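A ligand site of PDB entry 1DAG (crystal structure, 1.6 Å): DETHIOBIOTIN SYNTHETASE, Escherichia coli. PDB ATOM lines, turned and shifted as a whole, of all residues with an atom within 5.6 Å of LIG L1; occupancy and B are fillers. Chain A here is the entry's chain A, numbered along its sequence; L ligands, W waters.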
ATOM      1  N   ASP A  10     -21.472 -19.241 -25.746  1.00  0.00           N
ATOM      2  CA  ASP A  10     -22.134 -20.458 -26.137  1.00  0.00           C
ATOM      3  C   ASP A  10     -21.526 -21.556 -25.230  1.00  0.00           C
ATOM      4  O   ASP A  10     -20.583 -21.324 -24.441  1.00  0.00           O
ATOM      5  CB  ASP A  10     -21.798 -20.758 -27.599  1.00  0.00           C
ATOM      6  CG  ASP A  10     -22.666 -21.820 -28.295  1.00  0.00           C
ATOM      7  OD1 ASP A  10     -23.661 -22.268 -27.709  1.00  0.00           O
ATOM      8  OD2 ASP A  10     -22.367 -22.185 -29.437  1.00  0.00           O
ATOM      9  N   THR A  11     -22.110 -22.761 -25.262  1.00  0.00           N
ATOM     10  CA  THR A  11     -21.474 -23.947 -24.699  1.00  0.00           C
ATOM     11  C   THR A  11     -20.255 -24.251 -25.613  1.00  0.00           C
ATOM     12  O   THR A  11     -20.230 -23.884 -26.786  1.00  0.00           O
ATOM     13  CB  THR A  11     -22.562 -25.060 -24.703  1.00  0.00           C
ATOM     14  OG1 THR A  11     -21.933 -26.164 -24.020  1.00  0.00           O
ATOM     15  CG2 THR A  11     -23.082 -25.423 -26.095  1.00  0.00           C
ATOM     16  N   GLU A  12     -19.217 -24.888 -25.070  1.00  0.00           N
ATOM     17  CA  GLU A  12     -17.973 -25.261 -25.762  1.00  0.00           C
ATOM     18  C   GLU A  12     -17.192 -24.137 -26.466  1.00  0.00           C
ATOM     19  O   GLU A  12     -16.770 -24.263 -27.610  1.00  0.00           O
ATOM     20  CB  GLU A  12     -18.235 -26.358 -26.814  1.00  0.00           C
ATOM     21  CG  GLU A  12     -18.864 -27.681 -26.323  1.00  0.00           C
ATOM     22  CD  GLU A  12     -18.025 -28.507 -25.362  1.00  0.00           C
ATOM     23  OE1 GLU A  12     -17.023 -29.106 -25.789  1.00  0.00           O
ATOM     24  OE2 GLU A  12     -18.402 -28.569 -24.193  1.00  0.00           O
ATOM     25  N   VAL A  13     -17.007 -22.976 -25.806  1.00  0.00           N
ATOM     26  CA  VAL A  13     -16.151 -21.885 -26.318  1.00  0.00           C
ATOM     27  C   VAL A  13     -14.854 -21.771 -25.540  1.00  0.00           C
ATOM     28  O   VAL A  13     -14.055 -20.866 -25.772  1.00  0.00           O
ATOM     29  CB  VAL A  13     -16.837 -20.470 -26.275  1.00  0.00           C
ATOM     30  CG1 VAL A  13     -17.908 -20.463 -27.361  1.00  0.00           C
ATOM     31  CG2 VAL A  13     -17.434 -20.144 -24.902  1.00  0.00           C
ATOM     32  N   GLY A  14     -14.666 -22.647 -24.534  1.00  0.00           N
ATOM     33  CA  GLY A  14     -13.425 -22.745 -23.772  1.00  0.00           C
ATOM     34  C   GLY A  14     -13.488 -22.046 -22.434  1.00  0.00           C
ATOM     35  O   GLY A  14     -12.487 -21.613 -21.884  1.00  0.00           O
ATOM     36  N   LYS A  15     -14.685 -21.956 -21.863  1.00  0.00           N
ATOM     37  CA  LYS A  15     -14.882 -21.285 -20.593  1.00  0.00           C
ATOM     38  C   LYS A  15     -14.022 -21.939 -19.502  1.00  0.00           C
ATOM     39  O   LYS A  15     -13.433 -21.269 -18.655  1.00  0.00           O
ATOM     40  CB  LYS A  15     -16.364 -21.388 -20.298  1.00  0.00           C
ATOM     41  CG  LYS A  15     -17.055 -20.906 -19.054  1.00  0.00           C
ATOM     42  CD  LYS A  15     -18.572 -20.985 -19.407  1.00  0.00           C
ATOM     43  CE  LYS A  15     -19.179 -22.394 -19.629  1.00  0.00           C
ATOM     44  NZ  LYS A  15     -19.576 -22.592 -21.033  1.00  0.00           N
ATOM     45  N   THR A  16     -13.806 -23.260 -19.548  1.00  0.00           N
ATOM     46  CA  THR A  16     -12.977 -23.863 -18.504  1.00  0.00           C
ATOM     47  C   THR A  16     -11.504 -23.557 -18.726  1.00  0.00           C
ATOM     48  O   THR A  16     -10.778 -23.342 -17.764  1.00  0.00           O
ATOM     49  CB  THR A  16     -13.240 -25.419 -18.488  1.00  0.00           C
ATOM     50  OG1 THR A  16     -14.630 -25.505 -18.107  1.00  0.00           O
ATOM     51  CG2 THR A  16     -12.344 -26.260 -17.573  1.00  0.00           C
ATOM     52  N   VAL A  17     -11.021 -23.473 -19.970  1.00  0.00           N
ATOM     53  CA  VAL A  17      -9.618 -23.146 -20.254  1.00  0.00           C
ATOM     54  C   VAL A  17      -9.383 -21.719 -19.711  1.00  0.00           C
ATOM     55  O   VAL A  17      -8.400 -21.492 -18.979  1.00  0.00           O
ATOM     56  CB  VAL A  17      -9.367 -23.228 -21.809  1.00  0.00           C
ATOM     57  CG1 VAL A  17      -7.991 -22.661 -22.224  1.00  0.00           C
ATOM     58  CG2 VAL A  17      -9.419 -24.709 -22.210  1.00  0.00           C
ATOM     59  N   ALA A  18     -10.270 -20.763 -20.032  1.00  0.00           N
ATOM     60  CA  ALA A  18     -10.147 -19.399 -19.522  1.00  0.00           C
ATOM     61  C   ALA A  18     -10.280 -19.338 -17.986  1.00  0.00           C
ATOM     62  O   ALA A  18      -9.547 -18.569 -17.345  1.00  0.00           O
ATOM     63  CB  ALA A  18     -11.209 -18.512 -20.124  1.00  0.00           C
ATOM     64  N   LYS A  37     -17.781 -25.237  -9.518  1.00  0.00           N
ATOM     65  CA  LYS A  37     -18.711 -25.499 -10.609  1.00  0.00           C
ATOM     66  C   LYS A  37     -19.961 -26.164  -9.954  1.00  0.00           C
ATOM     67  O   LYS A  37     -19.988 -27.386  -9.743  1.00  0.00           O
ATOM     68  CB  LYS A  37     -18.047 -26.441 -11.639  1.00  0.00           C
ATOM     69  CG  LYS A  37     -18.931 -26.407 -12.898  1.00  0.00           C
ATOM     70  CD  LYS A  37     -18.392 -27.239 -14.037  1.00  0.00           C
ATOM     71  CE  LYS A  37     -19.373 -27.394 -15.223  1.00  0.00           C
ATOM     72  NZ  LYS A  37     -19.382 -26.258 -16.121  1.00  0.00           N
ATOM     73  N   ASP A  54     -14.394 -30.888 -16.405  1.00  0.00           N
ATOM     74  CA  ASP A  54     -14.273 -29.474 -16.167  1.00  0.00           C
ATOM     75  C   ASP A  54     -14.119 -29.151 -14.697  1.00  0.00           C
ATOM     76  O   ASP A  54     -13.223 -28.388 -14.329  1.00  0.00           O
ATOM     77  CB  ASP A  54     -15.499 -28.778 -16.757  1.00  0.00           C
ATOM     78  CG  ASP A  54     -15.490 -28.848 -18.298  1.00  0.00           C
ATOM     79  OD1 ASP A  54     -14.511 -29.308 -18.905  1.00  0.00           O
ATOM     80  OD2 ASP A  54     -16.457 -28.400 -18.914  1.00  0.00           O
ATOM     81  N   GLU A 115     -18.021 -21.130 -12.049  1.00  0.00           N
ATOM     82  CA  GLU A 115     -18.202 -21.393 -13.472  1.00  0.00           C
ATOM     83  C   GLU A 115     -19.617 -21.930 -13.633  1.00  0.00           C
ATOM     84  O   GLU A 115     -20.018 -22.815 -12.885  1.00  0.00           O
ATOM     85  CB  GLU A 115     -17.174 -22.433 -13.918  1.00  0.00           C
ATOM     86  CG  GLU A 115     -17.079 -22.587 -15.408  1.00  0.00           C
ATOM     87  CD  GLU A 115     -16.128 -23.671 -15.945  1.00  0.00           C
ATOM     88  OE1 GLU A 115     -14.918 -23.541 -15.874  1.00  0.00           O
ATOM     89  OE2 GLU A 115     -16.601 -24.656 -16.494  1.00  0.00           O
ATOM     90  N   GLY A 116     -20.462 -21.385 -14.496  1.00  0.00           N
ATOM     91  CA  GLY A 116     -21.789 -21.951 -14.693  1.00  0.00           C
ATOM     92  C   GLY A 116     -21.685 -23.130 -15.653  1.00  0.00           C
ATOM     93  O   GLY A 116     -20.601 -23.679 -15.886  1.00  0.00           O
ATOM     94  N   ALA A 117     -22.839 -23.564 -16.185  1.00  0.00           N
ATOM     95  CA  ALA A 117     -22.843 -24.645 -17.173  1.00  0.00           C
ATOM     96  C   ALA A 117     -23.487 -24.048 -18.427  1.00  0.00           C
ATOM     97  O   ALA A 117     -24.432 -23.262 -18.325  1.00  0.00           O
ATOM     98  CB  ALA A 117     -23.648 -25.837 -16.620  1.00  0.00           C
ATOM     99  N   GLY A 118     -22.947 -24.326 -19.615  1.00  0.00           N
ATOM    100  CA  GLY A 118     -23.435 -23.753 -20.887  1.00  0.00           C
ATOM    101  C   GLY A 118     -23.332 -22.222 -20.896  1.00  0.00           C
ATOM    102  O   GLY A 118     -22.372 -21.646 -20.359  1.00  0.00           O
ATOM    103  N   ASN A 175     -10.848 -16.057 -26.366  1.00  0.00           N
ATOM    104  CA  ASN A 175     -10.261 -17.369 -26.437  1.00  0.00           C
ATOM    105  C   ASN A 175     -10.191 -17.808 -27.883  1.00  0.00           C
ATOM    106  O   ASN A 175     -11.191 -17.798 -28.625  1.00  0.00           O
ATOM    107  CB  ASN A 175     -11.083 -18.353 -25.635  1.00  0.00           C
ATOM    108  CG  ASN A 175     -10.406 -19.705 -25.489  1.00  0.00           C
ATOM    109  OD1 ASN A 175      -9.172 -19.836 -25.533  1.00  0.00           O
ATOM    110  ND2 ASN A 175     -11.155 -20.782 -25.338  1.00  0.00           N
ATOM    111  N   ASP A 176      -9.001 -18.158 -28.346  1.00  0.00           N
ATOM    112  CA  ASP A 176      -8.828 -18.520 -29.727  1.00  0.00           C
ATOM    113  C   ASP A 176      -9.060 -20.003 -29.923  1.00  0.00           C
ATOM    114  O   ASP A 176      -8.220 -20.879 -29.689  1.00  0.00           O
ATOM    115  CB  ASP A 176      -7.438 -18.127 -30.170  1.00  0.00           C
ATOM    116  CG  ASP A 176      -7.095 -16.668 -30.036  1.00  0.00           C
ATOM    117  OD1 ASP A 176      -7.972 -15.804 -29.927  1.00  0.00           O
ATOM    118  OD2 ASP A 176      -5.903 -16.389 -30.072  1.00  0.00           O
ATOM    119  N   VAL A 177     -10.296 -20.270 -30.334  1.00  0.00           N
ATOM    120  CA  VAL A 177     -10.708 -21.653 -30.551  1.00  0.00           C
ATOM    121  C   VAL A 177     -10.240 -22.207 -31.905  1.00  0.00           C
ATOM    122  O   VAL A 177     -10.163 -23.431 -32.096  1.00  0.00           O
ATOM    123  CB  VAL A 177     -12.293 -21.738 -30.367  1.00  0.00           C
ATOM    124  CG1 VAL A 177     -12.571 -21.438 -28.908  1.00  0.00           C
ATOM    125  CG2 VAL A 177     -13.084 -20.764 -31.260  1.00  0.00           C
ATOM    126  N   ILE A 203      -6.223 -15.799 -24.967  1.00  0.00           N
ATOM    127  CA  ILE A 203      -5.548 -17.087 -24.903  1.00  0.00           C
ATOM    128  C   ILE A 203      -5.422 -17.598 -26.329  1.00  0.00           C
ATOM    129  O   ILE A 203      -6.396 -17.629 -27.085  1.00  0.00           O
ATOM    130  CB  ILE A 203      -6.357 -18.077 -23.994  1.00  0.00           C
ATOM    131  CG1 ILE A 203      -6.348 -17.479 -22.552  1.00  0.00           C
ATOM    132  CG2 ILE A 203      -5.716 -19.481 -23.930  1.00  0.00           C
ATOM    133  CD1 ILE A 203      -7.659 -17.668 -21.820  1.00  0.00           C
ATOM    134  N   PRO A 204      -4.203 -17.920 -26.764  1.00  0.00           N
ATOM    135  CA  PRO A 204      -3.937 -18.415 -28.117  1.00  0.00           C
ATOM    136  C   PRO A 204      -4.443 -19.834 -28.348  1.00  0.00           C
ATOM    137  O   PRO A 204      -4.717 -20.533 -27.365  1.00  0.00           O
ATOM    138  CB  PRO A 204      -2.414 -18.270 -28.246  1.00  0.00           C
ATOM    139  CG  PRO A 204      -1.896 -18.439 -26.840  1.00  0.00           C
ATOM    140  CD  PRO A 204      -2.973 -17.811 -25.960  1.00  0.00           C
ATOM    141  N   TRP A 205      -4.524 -20.283 -29.612  1.00  0.00           N
ATOM    142  CA  TRP A 205      -5.003 -21.608 -29.987  1.00  0.00           C
ATOM    143  C   TRP A 205      -3.931 -22.565 -29.477  1.00  0.00           C
ATOM    144  O   TRP A 205      -2.769 -22.473 -29.864  1.00  0.00           O
ATOM    145  CB  TRP A 205      -5.157 -21.698 -31.552  1.00  0.00           C
ATOM    146  CG  TRP A 205      -5.413 -23.111 -32.118  1.00  0.00           C
ATOM    147  CD1 TRP A 205      -6.607 -23.757 -31.821  1.00  0.00           C
ATOM    148  CD2 TRP A 205      -4.524 -23.897 -32.851  1.00  0.00           C
ATOM    149  NE1 TRP A 205      -6.466 -24.958 -32.347  1.00  0.00           N
ATOM    150  CE2 TRP A 205      -5.279 -25.106 -32.965  1.00  0.00           C
ATOM    151  CE3 TRP A 205      -3.241 -23.876 -33.450  1.00  0.00           C
ATOM    152  CZ2 TRP A 205      -4.775 -26.241 -33.635  1.00  0.00           C
ATOM    153  CZ3 TRP A 205      -2.755 -25.002 -34.111  1.00  0.00           C
ATOM    154  CH2 TRP A 205      -3.504 -26.165 -34.205  1.00  0.00           C
ATOM    155  N   LEU A 206      -4.276 -23.453 -28.541  1.00  0.00           N
ATOM    156  CA  LEU A 206      -3.325 -24.407 -27.986  1.00  0.00           C
ATOM    157  C   LEU A 206      -3.860 -25.795 -28.297  1.00  0.00           C
ATOM    158  O   LEU A 206      -4.709 -26.350 -27.607  1.00  0.00           O
ATOM    159  CB  LEU A 206      -3.204 -24.184 -26.453  1.00  0.00           C
ATOM    160  CG  LEU A 206      -2.704 -22.801 -25.999  1.00  0.00           C
ATOM    161  CD1 LEU A 206      -3.189 -22.469 -24.608  1.00  0.00           C
ATOM    162  CD2 LEU A 206      -1.186 -22.778 -26.217  1.00  0.00           C
ATOM    163  N   ALA A 207      -3.363 -26.349 -29.387  1.00  0.00           N
ATOM    164  CA  ALA A 207      -3.726 -27.669 -29.847  1.00  0.00           C
ATOM    165  C   ALA A 207      -3.858 -28.791 -28.792  1.00  0.00           C
ATOM    166  O   ALA A 207      -4.912 -29.373 -28.627  1.00  0.00           O
ATOM    167  CB  ALA A 207      -2.692 -28.066 -30.903  1.00  0.00           C
ATOM    168  N   PRO A 210      -5.136 -27.756 -23.546  1.00  0.00           N
ATOM    169  CA  PRO A 210      -4.944 -26.368 -23.111  1.00  0.00           C
ATOM    170  C   PRO A 210      -5.325 -26.053 -21.675  1.00  0.00           C
ATOM    171  O   PRO A 210      -4.920 -25.014 -21.152  1.00  0.00           O
ATOM    172  CB  PRO A 210      -5.734 -25.563 -24.140  1.00  0.00           C
ATOM    173  CG  PRO A 210      -6.828 -26.477 -24.594  1.00  0.00           C
ATOM    174  CD  PRO A 210      -6.059 -27.797 -24.683  1.00  0.00           C
ATOM    175  N   GLU A 211      -6.103 -26.896 -20.967  1.00  0.00           N
ATOM    176  CA  GLU A 211      -6.425 -26.674 -19.556  1.00  0.00           C
ATOM    177  C   GLU A 211      -5.313 -27.106 -18.564  1.00  0.00           C
ATOM    178  O   GLU A 211      -5.284 -26.703 -17.387  1.00  0.00           O
ATOM    179  CB  GLU A 211      -7.789 -27.352 -19.252  1.00  0.00           C
ATOM    180  CG  GLU A 211      -8.162 -28.815 -19.493  1.00  0.00           C
ATOM    181  CD  GLU A 211      -7.258 -29.617 -20.419  1.00  0.00           C
ATOM    182  OE1 GLU A 211      -7.366 -29.510 -21.655  1.00  0.00           O
ATOM    183  OE2 GLU A 211      -6.441 -30.354 -19.876  1.00  0.00           O
HETATM  184  P1  LIG L   1     -19.429 -26.348 -21.261  1.00  0.00           P
HETATM  185  O1  LIG L   1     -20.325 -25.529 -22.119  1.00  0.00           O
HETATM  186  O2  LIG L   1     -19.368 -25.644 -19.806  1.00  0.00           O
HETATM  187  O3  LIG L   1     -19.852 -27.762 -21.183  1.00  0.00           O
HETATM  188  P2  LIG L   1     -16.571 -24.915 -21.947  1.00  0.00           P
HETATM  189  O4  LIG L   1     -16.176 -24.714 -20.530  1.00  0.00           O
HETATM  190  O5  LIG L   1     -17.246 -23.721 -22.564  1.00  0.00           O
HETATM  191  C1  LIG L   1     -17.729 -26.334 -21.962  1.00  0.00           C
HETATM  192  P3  LIG L   1     -13.913 -26.057 -22.597  1.00  0.00           P
HETATM  193  O6  LIG L   1     -14.054 -27.376 -22.004  1.00  0.00           O
HETATM  194  O7  LIG L   1     -12.995 -25.194 -21.814  1.00  0.00           O
HETATM  195  O8  LIG L   1     -15.328 -25.336 -22.820  1.00  0.00           O
HETATM  196  O9  LIG L   1     -13.447 -26.165 -24.129  1.00  0.00           O
HETATM  197  C2  LIG L   1     -14.344 -26.769 -25.091  1.00  0.00           C
HETATM  198  C3  LIG L   1     -13.456 -27.446 -26.125  1.00  0.00           C
HETATM  199  O10 LIG L   1     -12.712 -26.434 -26.837  1.00  0.00           O
HETATM  200  C4  LIG L   1     -12.440 -28.395 -25.472  1.00  0.00           C
HETATM  201  O11 LIG L   1     -12.278 -29.602 -26.222  1.00  0.00           O
HETATM  202  C5  LIG L   1     -11.154 -27.587 -25.401  1.00  0.00           C
HETATM  203  O12 LIG L   1      -9.967 -28.405 -25.424  1.00  0.00           O
HETATM  204  C6  LIG L   1     -11.283 -26.663 -26.616  1.00  0.00           C
HETATM  205  N1  LIG L   1     -10.531 -25.374 -26.442  1.00  0.00           N
HETATM  206  C7  LIG L   1     -10.897 -24.374 -25.610  1.00  0.00           C
HETATM  207  N2  LIG L   1      -9.964 -23.428 -25.643  1.00  0.00           N
HETATM  208  C8  LIG L   1      -9.006 -23.805 -26.488  1.00  0.00           C
HETATM  209  C9  LIG L   1      -7.821 -23.235 -26.909  1.00  0.00           C
HETATM  210  N3  LIG L   1      -7.370 -22.078 -26.422  1.00  0.00           N
HETATM  211  N4  LIG L   1      -7.080 -23.906 -27.823  1.00  0.00           N
HETATM  212  C10 LIG L   1      -7.467 -25.109 -28.301  1.00  0.00           C
HETATM  213  N5  LIG L   1      -8.590 -25.667 -27.881  1.00  0.00           N
HETATM  214  C11 LIG L   1      -9.401 -25.033 -26.977  1.00  0.00           C
HETATM  215  C1  LG2 L   2     -29.034 -24.781 -23.634  1.00  0.00           C
HETATM  216  O1  LG2 L   2     -29.477 -25.397 -24.631  1.00  0.00           O
HETATM  217  O2  LG2 L   2     -28.925 -23.547 -23.634  1.00  0.00           O
HETATM  218  C2  LG2 L   2     -28.606 -25.543 -22.378  1.00  0.00           C
HETATM  219  C3  LG2 L   2     -27.166 -26.042 -22.568  1.00  0.00           C
HETATM  220  C4  LG2 L   2     -26.609 -26.688 -21.302  1.00  0.00           C
HETATM  221  C5  LG2 L   2     -25.167 -27.131 -21.535  1.00  0.00           C
HETATM  222  C6  LG2 L   2     -24.492 -27.776 -20.323  1.00  0.00           C
HETATM  223  C7  LG2 L   2     -23.030 -28.291 -20.572  1.00  0.00           C
HETATM  224  C8  LG2 L   2     -22.912 -29.254 -21.797  1.00  0.00           C
HETATM  225  C9  LG2 L   2     -23.673 -30.581 -21.601  1.00  0.00           C
HETATM  226  N1  LG2 L   2     -22.541 -29.034 -19.390  1.00  0.00           N
HETATM  227  C10 LG2 L   2     -21.679 -28.561 -18.490  1.00  0.00           C
HETATM  228  O3  LG2 L   2     -21.283 -27.388 -18.594  1.00  0.00           O
HETATM  229  O4  LG2 L   2     -21.308 -29.310 -17.587  1.00  0.00           O
HETATM  230  N2  LG2 L   2     -21.520 -29.596 -22.072  1.00  0.00           N
HETATM  231  O   HOH W   1      -9.771 -28.767 -22.799  1.00  0.00           O
HETATM  232  O   HOH W   2     -15.315 -29.322 -21.307  1.00  0.00           O
HETATM  233  O   HOH W   3     -11.445 -27.502 -20.742  1.00  0.00           O
HETATM  234  O   HOH W   4     -12.880 -30.381 -22.142  1.00  0.00           O
HETATM  235  O   HOH W   5     -18.006 -29.663 -21.846  1.00  0.00           O
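The side-chain amide nitrogen (ND2) of Asn 175 lies within hydrogen-bond range of the backbone carbonyl oxygen (O) of Val 13. O of Ile 203 lies within hydrogen-bond range of N of Asp 176 (2.9 Å). OG1 of Thr 16 sits at hydrogen-bond distance from OE2 of Glu 115, 2.7 Å away. The side-chain amino group (NZ) of Lys 37 lies within salt-bridge range of the side-chain carboxylate (OE2) of Glu 115. O of Gly 116 sits at hydrogen-bond distance from NZ of Lys 37 (2.9 Å). The backbone carbonyl oxygen of Gly 118 sits at hydrogen-bond distance from the side-chain amino group of Lys 15, 3.0 Å away.
Water W2 bridges an oxygen (O6) of LIG L1 (2.4 Å) and the side-chain carboxylate (OD1) of Asp 54 (2.5 Å). Water W1 lies within hydrogen-bond range of O12 of LIG L1 (2.7 Å) and OE1 of Glu 211 (2.8 Å). Water W5 lies within hydrogen-bond range of OE2 of Glu 12 (2.6 Å) and O3 of LIG L1 (2.7 Å).
A nitrogen (N2) of LG2 L2 sits at hydrogen-bond distance from an oxygen (O3) of LIG L1, 2.6 Å away.
Asp 54 touches LIG L1 (OD1 to O6, 3.7 Å). Gly 118 touches LIG L1. Asp 176 touches LIG L1 (O to N3, 3.6 Å). Ile 203 touches LIG L1. Trp 205 touches LIG L1 (CA to N4, 3.8 Å). CG of Pro 210 touches O12 of LIG L1, 3.8 Å away. Hydrophobic or aromatic side chains within 4 Å of LIG L1: Val 17, Ile 203, Trp 205 and Pro 210. The nearest printed residue that does not touch LIG L1 is Glu 115 (4.1 Å).
The backbone NH (N) of Gly 14 is in hydrogen-bond range of an oxygen (O8) of LIG L1. The backbone NH of Glu 12 lies within hydrogen-bond range of an oxygen (O1) of LIG L1, 3.2 Å away. The backbone NH of Leu 206 is in hydrogen-bond range of a nitrogen (N4) of LIG L1, 2.9 Å away. OG1 of Thr 11 lies within hydrogen-bond range of O1 of LIG L1. N of Thr 16 sits at hydrogen-bond distance from O4 of LIG L1 (2.9 Å). N2 of LG2 L2 is in salt-bridge range of OE2 of Glu 12, 3.9 Å away. The side-chain amide nitrogen (ND2) of Asn 175 is in hydrogen-bond range of a nitrogen (N2) of LIG L1 (2.9 Å). An oxygen (O5) of LIG L1 is in salt-bridge range of the side-chain amino group (NZ) of Lys 15, at 3.0 Å. NZ of Lys 37 lies within salt-bridge range of O2 of LIG L1 (3.7 Å). N of Val 13 sits at hydrogen-bond distance from O5 of LIG L1 (3.3 Å). The side-chain amino group of Lys 37 is in salt-bridge range of an oxygen (O3) of LG2 L2 (3.3 Å). The backbone carbonyl oxygen (O) of Pro 204 lies within hydrogen-bond range of a nitrogen (N3) of LIG L1, at 3.2 Å. The backbone NH (N) of Lys 15 lies within hydrogen-bond range of an oxygen (O5) of LIG L1, 3.2 Å away. An oxygen (O4) of LIG L1 is in hydrogen-bond range of the side-chain hydroxyl (OG1) of Thr 16 (3.0 Å). An oxygen (O7) of LIG L1 is in hydrogen-bond range of the backbone NH (N) of Val 17 (3.2 Å).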
